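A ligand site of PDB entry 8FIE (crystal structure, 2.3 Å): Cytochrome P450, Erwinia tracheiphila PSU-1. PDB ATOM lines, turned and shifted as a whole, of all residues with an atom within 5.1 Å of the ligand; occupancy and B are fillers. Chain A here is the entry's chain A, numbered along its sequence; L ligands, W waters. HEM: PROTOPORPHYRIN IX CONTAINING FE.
The side-chain sulfur (SG) of Cys 388 binds an iron atom (FE) of the ligand.
NE2 of His 114 is in hydrogen-bond range of O2D of the ligand (2.7 Å).
NH2 of Arg 320 is in salt-bridge range of O1A of the ligand, at 2.7 Å.
A ring nitrogen (ND1) of His 386 sits at hydrogen-bond distance from an oxygen (O1D) of the ligand.
An oxygen (O2D) of the ligand lies within salt-bridge range of the guanidinium group (NH1) of Arg 118, at 2.7 Å.
The backbone carbonyl oxygen (O) of Phe 381 is in hydrogen-bond range of the backbone NH (N) of Cys 388 (2.9 Å).
The backbone NH (N) of Gly 390 lies close to the side-chain sulfur (SG) of Cys 388 (3.3 Å).
A ring nitrogen (ND1) of His 386 lies within hydrogen-bond range of a ring nitrogen (NE2) of His 114 (3.5 Å).
A ring nitrogen (NE2) of His 114 sits close to the backbone carbonyl oxygen of Ile 385, 3.4 Å away.
The guanidinium group (NH1) of Arg 320 sits at hydrogen-bond distance from the backbone carbonyl oxygen (O) of Ile 318, at 3.5 Å.
The guanidinium group (NH1) of Arg 118 sits at hydrogen-bond distance from the backbone carbonyl oxygen (O) of Phe 387.
The side-chain hydroxyl of Thr 270 lies within hydrogen-bond range of the backbone carbonyl oxygen of Gly 266, 2.8 Å away.
The side-chain hydroxyl (OG) of Ser 380 sits at hydrogen-bond distance from the backbone carbonyl oxygen (O) of Leu 307 (2.5 Å).
NC of the ligand sits close to O of Gly 266, 3.1 Å away.
O of Ile 385 sits close to O2D of the ligand, at 3.4 Å.
Residues that only touch the ligand: Leu 106, Ala 107, Phe 125, Phe 173, Ile 263, Gly 267, Thr 270, Thr 271, Met 274, Ser 316, Ile 318, Leu 343, Ser 380, Phe 381, Gly 382, Phe 387, Leu 389, Gly 390 and Ala 394.
Within 4 Å of the ligand: Leu 106, Ala 107, His 114, Arg 118, Phe 125, Phe 173, Ile 263, Gly 266, Gly 267, Thr 270, Thr 271, Met 274, Ser 316, Ile 318, Arg 320, Leu 343, Ser 380, Phe 381, Gly 382, Ile 385, His 386, Phe 387, Cys 388, Leu 389, Gly 390 and Ala 394.
The nearest printed residue that does not touch the ligand is Leu 71 (4.1 Å).
Water W1 lies within hydrogen-bond range of OG1 of Thr 271 (2.4 Å) and O of Gly 267 (2.8 Å).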
ATOM      1  N   LEU A  71     -12.226  12.200 -34.520  1.00  0.00           N
ATOM      2  CA  LEU A  71     -13.428  11.375 -34.507  1.00  0.00           C
ATOM      3  C   LEU A  71     -14.004  11.214 -35.903  1.00  0.00           C
ATOM      4  O   LEU A  71     -14.416  10.110 -36.295  1.00  0.00           O
ATOM      5  CB  LEU A  71     -14.483  11.972 -33.569  1.00  0.00           C
ATOM      6  CG  LEU A  71     -14.192  11.907 -32.075  1.00  0.00           C
ATOM      7  CD1 LEU A  71     -15.175  12.777 -31.313  1.00  0.00           C
ATOM      8  CD2 LEU A  71     -14.255  10.475 -31.555  1.00  0.00           C
ATOM      9  N   LEU A 106     -19.314  -3.977 -31.750  1.00  0.00           N
ATOM     10  CA  LEU A 106     -19.316  -2.907 -32.739  1.00  0.00           C
ATOM     11  C   LEU A 106     -18.241  -1.866 -32.450  1.00  0.00           C
ATOM     12  O   LEU A 106     -17.578  -1.365 -33.359  1.00  0.00           O
ATOM     13  CB  LEU A 106     -20.704  -2.272 -32.753  1.00  0.00           C
ATOM     14  CG  LEU A 106     -21.121  -1.318 -33.869  1.00  0.00           C
ATOM     15  CD1 LEU A 106     -21.010  -1.966 -35.236  1.00  0.00           C
ATOM     16  CD2 LEU A 106     -22.563  -0.895 -33.591  1.00  0.00           C
ATOM     17  N   ALA A 107     -18.062  -1.519 -31.163  1.00  0.00           N
ATOM     18  CA  ALA A 107     -17.110  -0.469 -30.808  1.00  0.00           C
ATOM     19  C   ALA A 107     -15.691  -0.833 -31.207  1.00  0.00           C
ATOM     20  O   ALA A 107     -14.878   0.056 -31.486  1.00  0.00           O
ATOM     21  CB  ALA A 107     -17.181  -0.202 -29.302  1.00  0.00           C
ATOM     22  N   HIS A 114     -17.817  -3.094 -39.612  1.00  0.00           N
ATOM     23  CA  HIS A 114     -18.566  -2.213 -38.726  1.00  0.00           C
ATOM     24  C   HIS A 114     -19.779  -1.623 -39.414  1.00  0.00           C
ATOM     25  O   HIS A 114     -20.806  -1.387 -38.766  1.00  0.00           O
ATOM     26  CB  HIS A 114     -17.661  -1.085 -38.220  1.00  0.00           C
ATOM     27  CG  HIS A 114     -18.390  -0.037 -37.442  1.00  0.00           C
ATOM     28  ND1 HIS A 114     -18.930   1.084 -38.035  1.00  0.00           N
ATOM     29  CD2 HIS A 114     -18.669   0.058 -36.122  1.00  0.00           C
ATOM     30  CE1 HIS A 114     -19.516   1.829 -37.110  1.00  0.00           C
ATOM     31  NE2 HIS A 114     -19.375   1.223 -35.944  1.00  0.00           N
ATOM     32  N   ARG A 118     -23.523  -2.093 -37.851  1.00  0.00           N
ATOM     33  CA  ARG A 118     -24.259  -0.879 -37.478  1.00  0.00           C
ATOM     34  C   ARG A 118     -25.564  -0.780 -38.242  1.00  0.00           C
ATOM     35  O   ARG A 118     -26.614  -0.458 -37.673  1.00  0.00           O
ATOM     36  CB  ARG A 118     -23.385   0.345 -37.736  1.00  0.00           C
ATOM     37  CG  ARG A 118     -24.028   1.657 -37.356  1.00  0.00           C
ATOM     38  CD  ARG A 118     -23.421   2.225 -36.094  1.00  0.00           C
ATOM     39  NE  ARG A 118     -24.100   3.435 -35.659  1.00  0.00           N
ATOM     40  CZ  ARG A 118     -23.732   4.158 -34.603  1.00  0.00           C
ATOM     41  NH1 ARG A 118     -22.697   3.790 -33.868  1.00  0.00           N
ATOM     42  NH2 ARG A 118     -24.413   5.251 -34.284  1.00  0.00           N
ATOM     43  N   PHE A 125     -33.240  -1.041 -34.006  1.00  0.00           N
ATOM     44  CA  PHE A 125     -33.055  -0.225 -32.795  1.00  0.00           C
ATOM     45  C   PHE A 125     -33.258   1.230 -33.199  1.00  0.00           C
ATOM     46  O   PHE A 125     -32.326   1.993 -33.420  1.00  0.00           O
ATOM     47  CB  PHE A 125     -31.683  -0.488 -32.187  1.00  0.00           C
ATOM     48  CG  PHE A 125     -31.462   0.190 -30.864  1.00  0.00           C
ATOM     49  CD1 PHE A 125     -32.404   0.123 -29.854  1.00  0.00           C
ATOM     50  CD2 PHE A 125     -30.290   0.895 -30.621  1.00  0.00           C
ATOM     51  CE1 PHE A 125     -32.188   0.744 -28.636  1.00  0.00           C
ATOM     52  CE2 PHE A 125     -30.066   1.520 -29.406  1.00  0.00           C
ATOM     53  CZ  PHE A 125     -31.013   1.450 -28.417  1.00  0.00           C
ATOM     54  N   PHE A 173     -33.156  -1.469 -19.893  1.00  0.00           N
ATOM     55  CA  PHE A 173     -32.583  -2.511 -20.745  1.00  0.00           C
ATOM     56  C   PHE A 173     -33.431  -3.781 -20.695  1.00  0.00           C
ATOM     57  O   PHE A 173     -33.658  -4.434 -21.714  1.00  0.00           O
ATOM     58  CB  PHE A 173     -31.144  -2.824 -20.332  1.00  0.00           C
ATOM     59  CG  PHE A 173     -30.090  -1.984 -21.020  1.00  0.00           C
ATOM     60  CD1 PHE A 173     -30.194  -1.664 -22.370  1.00  0.00           C
ATOM     61  CD2 PHE A 173     -28.994  -1.519 -20.312  1.00  0.00           C
ATOM     62  CE1 PHE A 173     -29.231  -0.898 -22.986  1.00  0.00           C
ATOM     63  CE2 PHE A 173     -28.023  -0.749 -20.931  1.00  0.00           C
ATOM     64  CZ  PHE A 173     -28.138  -0.445 -22.270  1.00  0.00           C
ATOM     65  N   GLY A 262     -22.600  -5.829 -26.377  1.00  0.00           N
ATOM     66  CA  GLY A 262     -22.007  -4.508 -26.518  1.00  0.00           C
ATOM     67  C   GLY A 262     -22.972  -3.392 -26.213  1.00  0.00           C
ATOM     68  O   GLY A 262     -22.568  -2.347 -25.687  1.00  0.00           O
ATOM     69  N   ILE A 263     -24.252  -3.582 -26.527  1.00  0.00           N
ATOM     70  CA  ILE A 263     -25.272  -2.618 -26.159  1.00  0.00           C
ATOM     71  C   ILE A 263     -25.336  -2.453 -24.646  1.00  0.00           C
ATOM     72  O   ILE A 263     -25.404  -1.336 -24.130  1.00  0.00           O
ATOM     73  CB  ILE A 263     -26.639  -3.042 -26.739  1.00  0.00           C
ATOM     74  CG1 ILE A 263     -26.662  -2.829 -28.258  1.00  0.00           C
ATOM     75  CG2 ILE A 263     -27.769  -2.297 -26.051  1.00  0.00           C
ATOM     76  CD1 ILE A 263     -27.869  -3.432 -28.949  1.00  0.00           C
ATOM     77  N   GLY A 266     -22.168  -0.682 -23.442  1.00  0.00           N
ATOM     78  CA  GLY A 266     -22.211   0.740 -23.730  1.00  0.00           C
ATOM     79  C   GLY A 266     -23.066   1.525 -22.746  1.00  0.00           C
ATOM     80  O   GLY A 266     -22.761   2.680 -22.458  1.00  0.00           O
ATOM     81  N   GLY A 267     -24.124   0.908 -22.226  1.00  0.00           N
ATOM     82  CA  GLY A 267     -25.002   1.533 -21.270  1.00  0.00           C
ATOM     83  C   GLY A 267     -24.718   1.200 -19.818  1.00  0.00           C
ATOM     84  O   GLY A 267     -25.526   1.540 -18.951  1.00  0.00           O
ATOM     85  N   THR A 270     -22.235   4.372 -17.659  1.00  0.00           N
ATOM     86  CA  THR A 270     -22.391   5.647 -18.375  1.00  0.00           C
ATOM     87  C   THR A 270     -23.721   6.316 -18.055  1.00  0.00           C
ATOM     88  O   THR A 270     -23.751   7.457 -17.566  1.00  0.00           O
ATOM     89  CB  THR A 270     -22.285   5.403 -19.885  1.00  0.00           C
ATOM     90  OG1 THR A 270     -23.239   4.414 -20.291  1.00  0.00           O
ATOM     91  CG2 THR A 270     -20.892   4.954 -20.277  1.00  0.00           C
ATOM     92  N   THR A 271     -24.824   5.635 -18.337  1.00  0.00           N
ATOM     93  CA  THR A 271     -26.150   6.210 -18.146  1.00  0.00           C
ATOM     94  C   THR A 271     -26.375   6.611 -16.691  1.00  0.00           C
ATOM     95  O   THR A 271     -26.861   7.714 -16.402  1.00  0.00           O
ATOM     96  CB  THR A 271     -27.217   5.212 -18.594  1.00  0.00           C
ATOM     97  OG1 THR A 271     -26.924   4.760 -19.922  1.00  0.00           O
ATOM     98  CG2 THR A 271     -28.600   5.850 -18.586  1.00  0.00           C
ATOM     99  N   MET A 274     -24.573   9.778 -16.003  1.00  0.00           N
ATOM    100  CA  MET A 274     -25.292  10.917 -16.583  1.00  0.00           C
ATOM    101  C   MET A 274     -26.451  11.343 -15.688  1.00  0.00           C
ATOM    102  O   MET A 274     -26.691  12.538 -15.507  1.00  0.00           O
ATOM    103  CB  MET A 274     -25.778  10.532 -17.976  1.00  0.00           C
ATOM    104  CG  MET A 274     -26.529  11.605 -18.751  1.00  0.00           C
ATOM    105  SD  MET A 274     -27.126  10.952 -20.328  1.00  0.00           S
ATOM    106  CE  MET A 274     -28.045  12.342 -20.986  1.00  0.00           C
ATOM    107  N   LEU A 307     -24.729  17.056 -20.315  1.00  0.00           N
ATOM    108  CA  LEU A 307     -23.741  16.261 -21.053  1.00  0.00           C
ATOM    109  C   LEU A 307     -22.499  17.084 -21.374  1.00  0.00           C
ATOM    110  O   LEU A 307     -21.377  16.543 -21.349  1.00  0.00           O
ATOM    111  CB  LEU A 307     -24.377  15.717 -22.331  1.00  0.00           C
ATOM    112  CG  LEU A 307     -25.424  14.615 -22.164  1.00  0.00           C
ATOM    113  CD1 LEU A 307     -26.318  14.540 -23.399  1.00  0.00           C
ATOM    114  CD2 LEU A 307     -24.755  13.269 -21.915  1.00  0.00           C
ATOM    115  N   PRO A 312     -20.175  12.286 -18.838  1.00  0.00           N
ATOM    116  CA  PRO A 312     -20.140  11.049 -18.039  1.00  0.00           C
ATOM    117  C   PRO A 312     -18.964  10.160 -18.420  1.00  0.00           C
ATOM    118  O   PRO A 312     -18.354   9.523 -17.545  1.00  0.00           O
ATOM    119  CB  PRO A 312     -21.497  10.396 -18.339  1.00  0.00           C
ATOM    120  CG  PRO A 312     -22.387  11.567 -18.678  1.00  0.00           C
ATOM    121  CD  PRO A 312     -21.491  12.492 -19.468  1.00  0.00           C
ATOM    122  N   ALA A 313     -18.623  10.104 -19.706  1.00  0.00           N
ATOM    123  CA  ALA A 313     -17.413   9.455 -20.183  1.00  0.00           C
ATOM    124  C   ALA A 313     -16.360  10.531 -20.440  1.00  0.00           C
ATOM    125  O   ALA A 313     -16.539  11.377 -21.320  1.00  0.00           O
ATOM    126  CB  ALA A 313     -17.682   8.654 -21.450  1.00  0.00           C
ATOM    127  N   SER A 316     -12.413   8.531 -24.682  1.00  0.00           N
ATOM    128  CA  SER A 316     -12.728   7.410 -25.552  1.00  0.00           C
ATOM    129  C   SER A 316     -12.031   6.155 -25.041  1.00  0.00           C
ATOM    130  O   SER A 316     -10.876   6.205 -24.611  1.00  0.00           O
ATOM    131  CB  SER A 316     -12.256   7.718 -26.979  1.00  0.00           C
ATOM    132  OG  SER A 316     -10.879   8.049 -27.006  1.00  0.00           O
ATOM    133  N   SER A 317     -12.741   5.033 -25.088  1.00  0.00           N
ATOM    134  CA  SER A 317     -12.117   3.738 -24.859  1.00  0.00           C
ATOM    135  C   SER A 317     -11.890   2.956 -26.152  1.00  0.00           C
ATOM    136  O   SER A 317     -11.229   1.924 -26.118  1.00  0.00           O
ATOM    137  CB  SER A 317     -12.961   2.888 -23.903  1.00  0.00           C
ATOM    138  OG  SER A 317     -14.334   2.936 -24.240  1.00  0.00           O
ATOM    139  N   ILE A 318     -12.412   3.442 -27.275  1.00  0.00           N
ATOM    140  CA  ILE A 318     -12.173   2.817 -28.574  1.00  0.00           C
ATOM    141  C   ILE A 318     -10.789   3.208 -29.056  1.00  0.00           C
ATOM    142  O   ILE A 318     -10.537   4.403 -29.294  1.00  0.00           O
ATOM    143  CB  ILE A 318     -13.247   3.238 -29.594  1.00  0.00           C
ATOM    144  CG1 ILE A 318     -14.636   2.773 -29.135  1.00  0.00           C
ATOM    145  CG2 ILE A 318     -12.921   2.665 -30.975  1.00  0.00           C
ATOM    146  CD1 ILE A 318     -15.762   3.268 -30.024  1.00  0.00           C
ATOM    147  N   ARG A 320      -7.921   4.148 -31.565  1.00  0.00           N
ATOM    148  CA  ARG A 320      -7.871   4.720 -32.911  1.00  0.00           C
ATOM    149  C   ARG A 320      -6.414   4.710 -33.361  1.00  0.00           C
ATOM    150  O   ARG A 320      -5.574   5.424 -32.800  1.00  0.00           O
ATOM    151  CB  ARG A 320      -8.439   6.139 -32.922  1.00  0.00           C
ATOM    152  CG  ARG A 320      -9.974   6.181 -32.873  1.00  0.00           C
ATOM    153  CD  ARG A 320     -10.508   7.595 -32.822  1.00  0.00           C
ATOM    154  NE  ARG A 320     -11.954   7.626 -33.017  1.00  0.00           N
ATOM    155  CZ  ARG A 320     -12.848   7.243 -32.100  1.00  0.00           C
ATOM    156  NH1 ARG A 320     -12.452   6.779 -30.932  1.00  0.00           N
ATOM    157  NH2 ARG A 320     -14.148   7.302 -32.373  1.00  0.00           N
ATOM    158  N   LEU A 343     -12.837  13.791 -24.390  1.00  0.00           N
ATOM    159  CA  LEU A 343     -14.133  14.367 -24.747  1.00  0.00           C
ATOM    160  C   LEU A 343     -14.531  15.480 -23.786  1.00  0.00           C
ATOM    161  O   LEU A 343     -14.973  16.547 -24.202  1.00  0.00           O
ATOM    162  CB  LEU A 343     -15.201  13.262 -24.756  1.00  0.00           C
ATOM    163  CG  LEU A 343     -14.952  12.065 -25.662  1.00  0.00           C
ATOM    164  CD1 LEU A 343     -15.987  10.968 -25.415  1.00  0.00           C
ATOM    165  CD2 LEU A 343     -14.974  12.493 -27.129  1.00  0.00           C
ATOM    166  N   LEU A 379     -19.282  16.733 -27.395  1.00  0.00           N
ATOM    167  CA  LEU A 379     -18.533  15.533 -27.740  1.00  0.00           C
ATOM    168  C   LEU A 379     -18.814  14.365 -26.805  1.00  0.00           C
ATOM    169  O   LEU A 379     -18.178  13.317 -26.940  1.00  0.00           O
ATOM    170  CB  LEU A 379     -17.043  15.859 -27.752  1.00  0.00           C
ATOM    171  CG  LEU A 379     -16.667  17.037 -28.669  1.00  0.00           C
ATOM    172  CD1 LEU A 379     -15.240  17.478 -28.410  1.00  0.00           C
ATOM    173  CD2 LEU A 379     -16.865  16.662 -30.129  1.00  0.00           C
ATOM    174  N   SER A 380     -19.765  14.511 -25.886  1.00  0.00           N
ATOM    175  CA  SER A 380     -20.003  13.494 -24.871  1.00  0.00           C
ATOM    176  C   SER A 380     -20.395  12.144 -25.473  1.00  0.00           C
ATOM    177  O   SER A 380     -20.231  11.119 -24.811  1.00  0.00           O
ATOM    178  CB  SER A 380     -21.093  13.950 -23.900  1.00  0.00           C
ATOM    179  OG  SER A 380     -20.897  15.291 -23.481  1.00  0.00           O
ATOM    180  N   PHE A 381     -20.917  12.146 -26.700  1.00  0.00           N
ATOM    181  CA  PHE A 381     -21.360  10.928 -27.364  1.00  0.00           C
ATOM    182  C   PHE A 381     -20.456  10.514 -28.516  1.00  0.00           C
ATOM    183  O   PHE A 381     -20.751   9.539 -29.206  1.00  0.00           O
ATOM    184  CB  PHE A 381     -22.791  11.110 -27.883  1.00  0.00           C
ATOM    185  CG  PHE A 381     -23.849  11.010 -26.816  1.00  0.00           C
ATOM    186  CD1 PHE A 381     -23.870   9.939 -25.933  1.00  0.00           C
ATOM    187  CD2 PHE A 381     -24.832  11.982 -26.715  1.00  0.00           C
ATOM    188  CE1 PHE A 381     -24.848   9.842 -24.974  1.00  0.00           C
ATOM    189  CE2 PHE A 381     -25.814  11.878 -25.740  1.00  0.00           C
ATOM    190  CZ  PHE A 381     -25.822  10.817 -24.876  1.00  0.00           C
ATOM    191  N   GLY A 382     -19.365  11.238 -28.737  1.00  0.00           N
ATOM    192  CA  GLY A 382     -18.492  10.971 -29.864  1.00  0.00           C
ATOM    193  C   GLY A 382     -18.933  11.731 -31.104  1.00  0.00           C
ATOM    194  O   GLY A 382     -19.681  12.716 -31.049  1.00  0.00           O
ATOM    195  N   ILE A 385     -18.449   7.619 -37.223  1.00  0.00           N
ATOM    196  CA  ILE A 385     -19.046   6.306 -37.433  1.00  0.00           C
ATOM    197  C   ILE A 385     -19.234   5.529 -36.144  1.00  0.00           C
ATOM    198  O   ILE A 385     -20.046   4.589 -36.118  1.00  0.00           O
ATOM    199  CB  ILE A 385     -18.217   5.487 -38.441  1.00  0.00           C
ATOM    200  CG1 ILE A 385     -16.891   5.044 -37.825  1.00  0.00           C
ATOM    201  CG2 ILE A 385     -17.950   6.311 -39.701  1.00  0.00           C
ATOM    202  CD1 ILE A 385     -16.041   4.223 -38.773  1.00  0.00           C
ATOM    203  N   HIS A 386     -18.512   5.861 -35.075  1.00  0.00           N
ATOM    204  CA  HIS A 386     -18.695   5.213 -33.786  1.00  0.00           C
ATOM    205  C   HIS A 386     -19.531   6.042 -32.819  1.00  0.00           C
ATOM    206  O   HIS A 386     -19.562   5.752 -31.619  1.00  0.00           O
ATOM    207  CB  HIS A 386     -17.331   4.896 -33.144  1.00  0.00           C
ATOM    208  CG  HIS A 386     -16.529   3.892 -33.914  1.00  0.00           C
ATOM    209  ND1 HIS A 386     -16.866   2.560 -33.969  1.00  0.00           N
ATOM    210  CD2 HIS A 386     -15.399   4.023 -34.645  1.00  0.00           C
ATOM    211  CE1 HIS A 386     -15.977   1.914 -34.709  1.00  0.00           C
ATOM    212  NE2 HIS A 386     -15.079   2.776 -35.125  1.00  0.00           N
ATOM    213  N   PHE A 387     -20.209   7.080 -33.322  1.00  0.00           N
ATOM    214  CA  PHE A 387     -21.121   7.868 -32.507  1.00  0.00           C
ATOM    215  C   PHE A 387     -22.026   6.949 -31.697  1.00  0.00           C
ATOM    216  O   PHE A 387     -22.545   5.956 -32.208  1.00  0.00           O
ATOM    217  CB  PHE A 387     -21.939   8.790 -33.399  1.00  0.00           C
ATOM    218  CG  PHE A 387     -22.951   9.614 -32.655  1.00  0.00           C
ATOM    219  CD1 PHE A 387     -24.276   9.210 -32.581  1.00  0.00           C
ATOM    220  CD2 PHE A 387     -22.575  10.795 -32.038  1.00  0.00           C
ATOM    221  CE1 PHE A 387     -25.198   9.972 -31.904  1.00  0.00           C
ATOM    222  CE2 PHE A 387     -23.504  11.558 -31.350  1.00  0.00           C
ATOM    223  CZ  PHE A 387     -24.816  11.147 -31.283  1.00  0.00           C
ATOM    224  N   CYS A 388     -22.211   7.293 -30.418  1.00  0.00           N
ATOM    225  CA  CYS A 388     -22.897   6.418 -29.482  1.00  0.00           C
ATOM    226  C   CYS A 388     -24.207   5.894 -30.045  1.00  0.00           C
ATOM    227  O   CYS A 388     -25.107   6.667 -30.387  1.00  0.00           O
ATOM    228  CB  CYS A 388     -23.156   7.164 -28.166  1.00  0.00           C
ATOM    229  SG  CYS A 388     -24.042   6.189 -26.926  1.00  0.00           S
ATOM    230  N   LEU A 389     -24.295   4.567 -30.151  1.00  0.00           N
ATOM    231  CA  LEU A 389     -25.523   3.933 -30.631  1.00  0.00           C
ATOM    232  C   LEU A 389     -26.702   4.214 -29.703  1.00  0.00           C
ATOM    233  O   LEU A 389     -27.847   4.269 -30.152  1.00  0.00           O
ATOM    234  CB  LEU A 389     -25.296   2.426 -30.765  1.00  0.00           C
ATOM    235  CG  LEU A 389     -26.395   1.574 -31.402  1.00  0.00           C
ATOM    236  CD1 LEU A 389     -26.461   1.836 -32.905  1.00  0.00           C
ATOM    237  CD2 LEU A 389     -26.165   0.097 -31.127  1.00  0.00           C
ATOM    238  N   GLY A 390     -26.424   4.411 -28.413  1.00  0.00           N
ATOM    239  CA  GLY A 390     -27.476   4.634 -27.436  1.00  0.00           C
ATOM    240  C   GLY A 390     -27.724   6.085 -27.063  1.00  0.00           C
ATOM    241  O   GLY A 390     -28.383   6.351 -26.067  1.00  0.00           O
ATOM    242  N   LEU A 393     -31.316   6.790 -26.605  1.00  0.00           N
ATOM    243  CA  LEU A 393     -31.835   6.047 -25.457  1.00  0.00           C
ATOM    244  C   LEU A 393     -31.453   6.723 -24.144  1.00  0.00           C
ATOM    245  O   LEU A 393     -32.287   6.853 -23.250  1.00  0.00           O
ATOM    246  CB  LEU A 393     -31.322   4.607 -25.503  1.00  0.00           C
ATOM    247  CG  LEU A 393     -31.748   3.685 -24.347  1.00  0.00           C
ATOM    248  CD1 LEU A 393     -33.255   3.639 -24.206  1.00  0.00           C
ATOM    249  CD2 LEU A 393     -31.182   2.290 -24.554  1.00  0.00           C
ATOM    250  N   ALA A 394     -30.203   7.166 -24.029  1.00  0.00           N
ATOM    251  CA  ALA A 394     -29.778   7.874 -22.821  1.00  0.00           C
ATOM    252  C   ALA A 394     -30.521   9.195 -22.661  1.00  0.00           C
ATOM    253  O   ALA A 394     -31.010   9.529 -21.577  1.00  0.00           O
ATOM    254  CB  ALA A 394     -28.260   8.112 -22.847  1.00  0.00           C
ATOM    255  N   GLN A 397     -34.141   8.660 -21.531  1.00  0.00           N
ATOM    256  CA  GLN A 397     -34.253   8.239 -20.140  1.00  0.00           C
ATOM    257  C   GLN A 397     -34.172   9.433 -19.197  1.00  0.00           C
ATOM    258  O   GLN A 397     -34.948   9.537 -18.238  1.00  0.00           O
ATOM    259  CB  GLN A 397     -33.163   7.228 -19.799  1.00  0.00           C
ATOM    260  CG  GLN A 397     -33.441   5.828 -20.346  1.00  0.00           C
ATOM    261  CD  GLN A 397     -32.449   4.797 -19.837  1.00  0.00           C
ATOM    262  OE1 GLN A 397     -32.307   4.607 -18.631  1.00  0.00           O
ATOM    263  NE2 GLN A 397     -31.769   4.121 -20.759  1.00  0.00           N
HETATM  264  CHA HEM L   1     -20.265   4.364 -28.292  1.00  0.00           C
HETATM  265  CHB HEM L   1     -20.857   7.635 -24.713  1.00  0.00           C
HETATM  266  CHC HEM L   1     -24.797   5.229 -23.243  1.00  0.00           C
HETATM  267  CHD HEM L   1     -24.172   1.928 -26.731  1.00  0.00           C
HETATM  268  C1A HEM L   1     -20.095   5.477 -27.487  1.00  0.00           C
HETATM  269  C2A HEM L   1     -19.103   6.525 -27.655  1.00  0.00           C
HETATM  270  C3A HEM L   1     -19.266   7.417 -26.672  1.00  0.00           C
HETATM  271  C4A HEM L   1     -20.371   6.980 -25.839  1.00  0.00           C
HETATM  272  CMA HEM L   1     -18.437   8.700 -26.443  1.00  0.00           C
HETATM  273  CAA HEM L   1     -18.054   6.576 -28.786  1.00  0.00           C
HETATM  274  CBA HEM L   1     -16.651   6.596 -28.183  1.00  0.00           C
HETATM  275  CGA HEM L   1     -15.601   6.674 -29.273  1.00  0.00           C
HETATM  276  O1A HEM L   1     -15.958   6.936 -30.453  1.00  0.00           O
HETATM  277  O2A HEM L   1     -14.408   6.486 -28.952  1.00  0.00           O
HETATM  278  C1B HEM L   1     -21.991   7.289 -24.010  1.00  0.00           C
HETATM  279  C2B HEM L   1     -22.601   8.024 -22.924  1.00  0.00           C
HETATM  280  C3B HEM L   1     -23.687   7.331 -22.532  1.00  0.00           C
HETATM  281  C4B HEM L   1     -23.800   6.161 -23.360  1.00  0.00           C
HETATM  282  CMB HEM L   1     -22.068   9.352 -22.319  1.00  0.00           C
HETATM  283  CAB HEM L   1     -24.725   7.632 -21.427  1.00  0.00           C
HETATM  284  CBB HEM L   1     -24.766   8.790 -20.770  1.00  0.00           C
HETATM  285  C1C HEM L   1     -25.032   4.186 -24.104  1.00  0.00           C
HETATM  286  C2C HEM L   1     -26.231   3.393 -24.172  1.00  0.00           C
HETATM  287  C3C HEM L   1     -26.080   2.485 -25.145  1.00  0.00           C
HETATM  288  C4C HEM L   1     -24.758   2.662 -25.716  1.00  0.00           C
HETATM  289  CMC HEM L   1     -27.487   3.586 -23.294  1.00  0.00           C
HETATM  290  CAC HEM L   1     -27.151   1.437 -25.537  1.00  0.00           C
HETATM  291  CBC HEM L   1     -27.218   0.983 -26.791  1.00  0.00           C
HETATM  292  C1D HEM L   1     -23.043   2.282 -27.439  1.00  0.00           C
HETATM  293  C2D HEM L   1     -22.459   1.528 -28.525  1.00  0.00           C
HETATM  294  C3D HEM L   1     -21.387   2.197 -28.960  1.00  0.00           C
HETATM  295  C4D HEM L   1     -21.247   3.405 -28.170  1.00  0.00           C
HETATM  296  CMD HEM L   1     -22.979   0.184 -29.084  1.00  0.00           C
HETATM  297  CAD HEM L   1     -20.450   1.766 -30.112  1.00  0.00           C
HETATM  298  CBD HEM L   1     -20.962   2.401 -31.403  1.00  0.00           C
HETATM  299  CGD HEM L   1     -20.022   2.122 -32.558  1.00  0.00           C
HETATM  300  O1D HEM L   1     -18.826   1.831 -32.314  1.00  0.00           O
HETATM  301  O2D HEM L   1     -20.475   2.202 -33.740  1.00  0.00           O
HETATM  302  NA  HEM L   1     -20.847   5.796 -26.370  1.00  0.00           N
HETATM  303  NB  HEM L   1     -22.755   6.165 -24.258  1.00  0.00           N
HETATM  304  NC  HEM L   1     -24.146   3.711 -25.050  1.00  0.00           N
HETATM  305  ND  HEM L   1     -22.283   3.416 -27.257  1.00  0.00           N
HETATM  306 FE   HEM L   1     -22.547   4.822 -25.796  1.00  0.00          FE
HETATM  307  O   HOH W   1     -27.793   2.529 -20.240  1.00  0.00           O
HETATM  308  O   HOH W   2     -21.244   3.892 -24.400  1.00  0.00           O
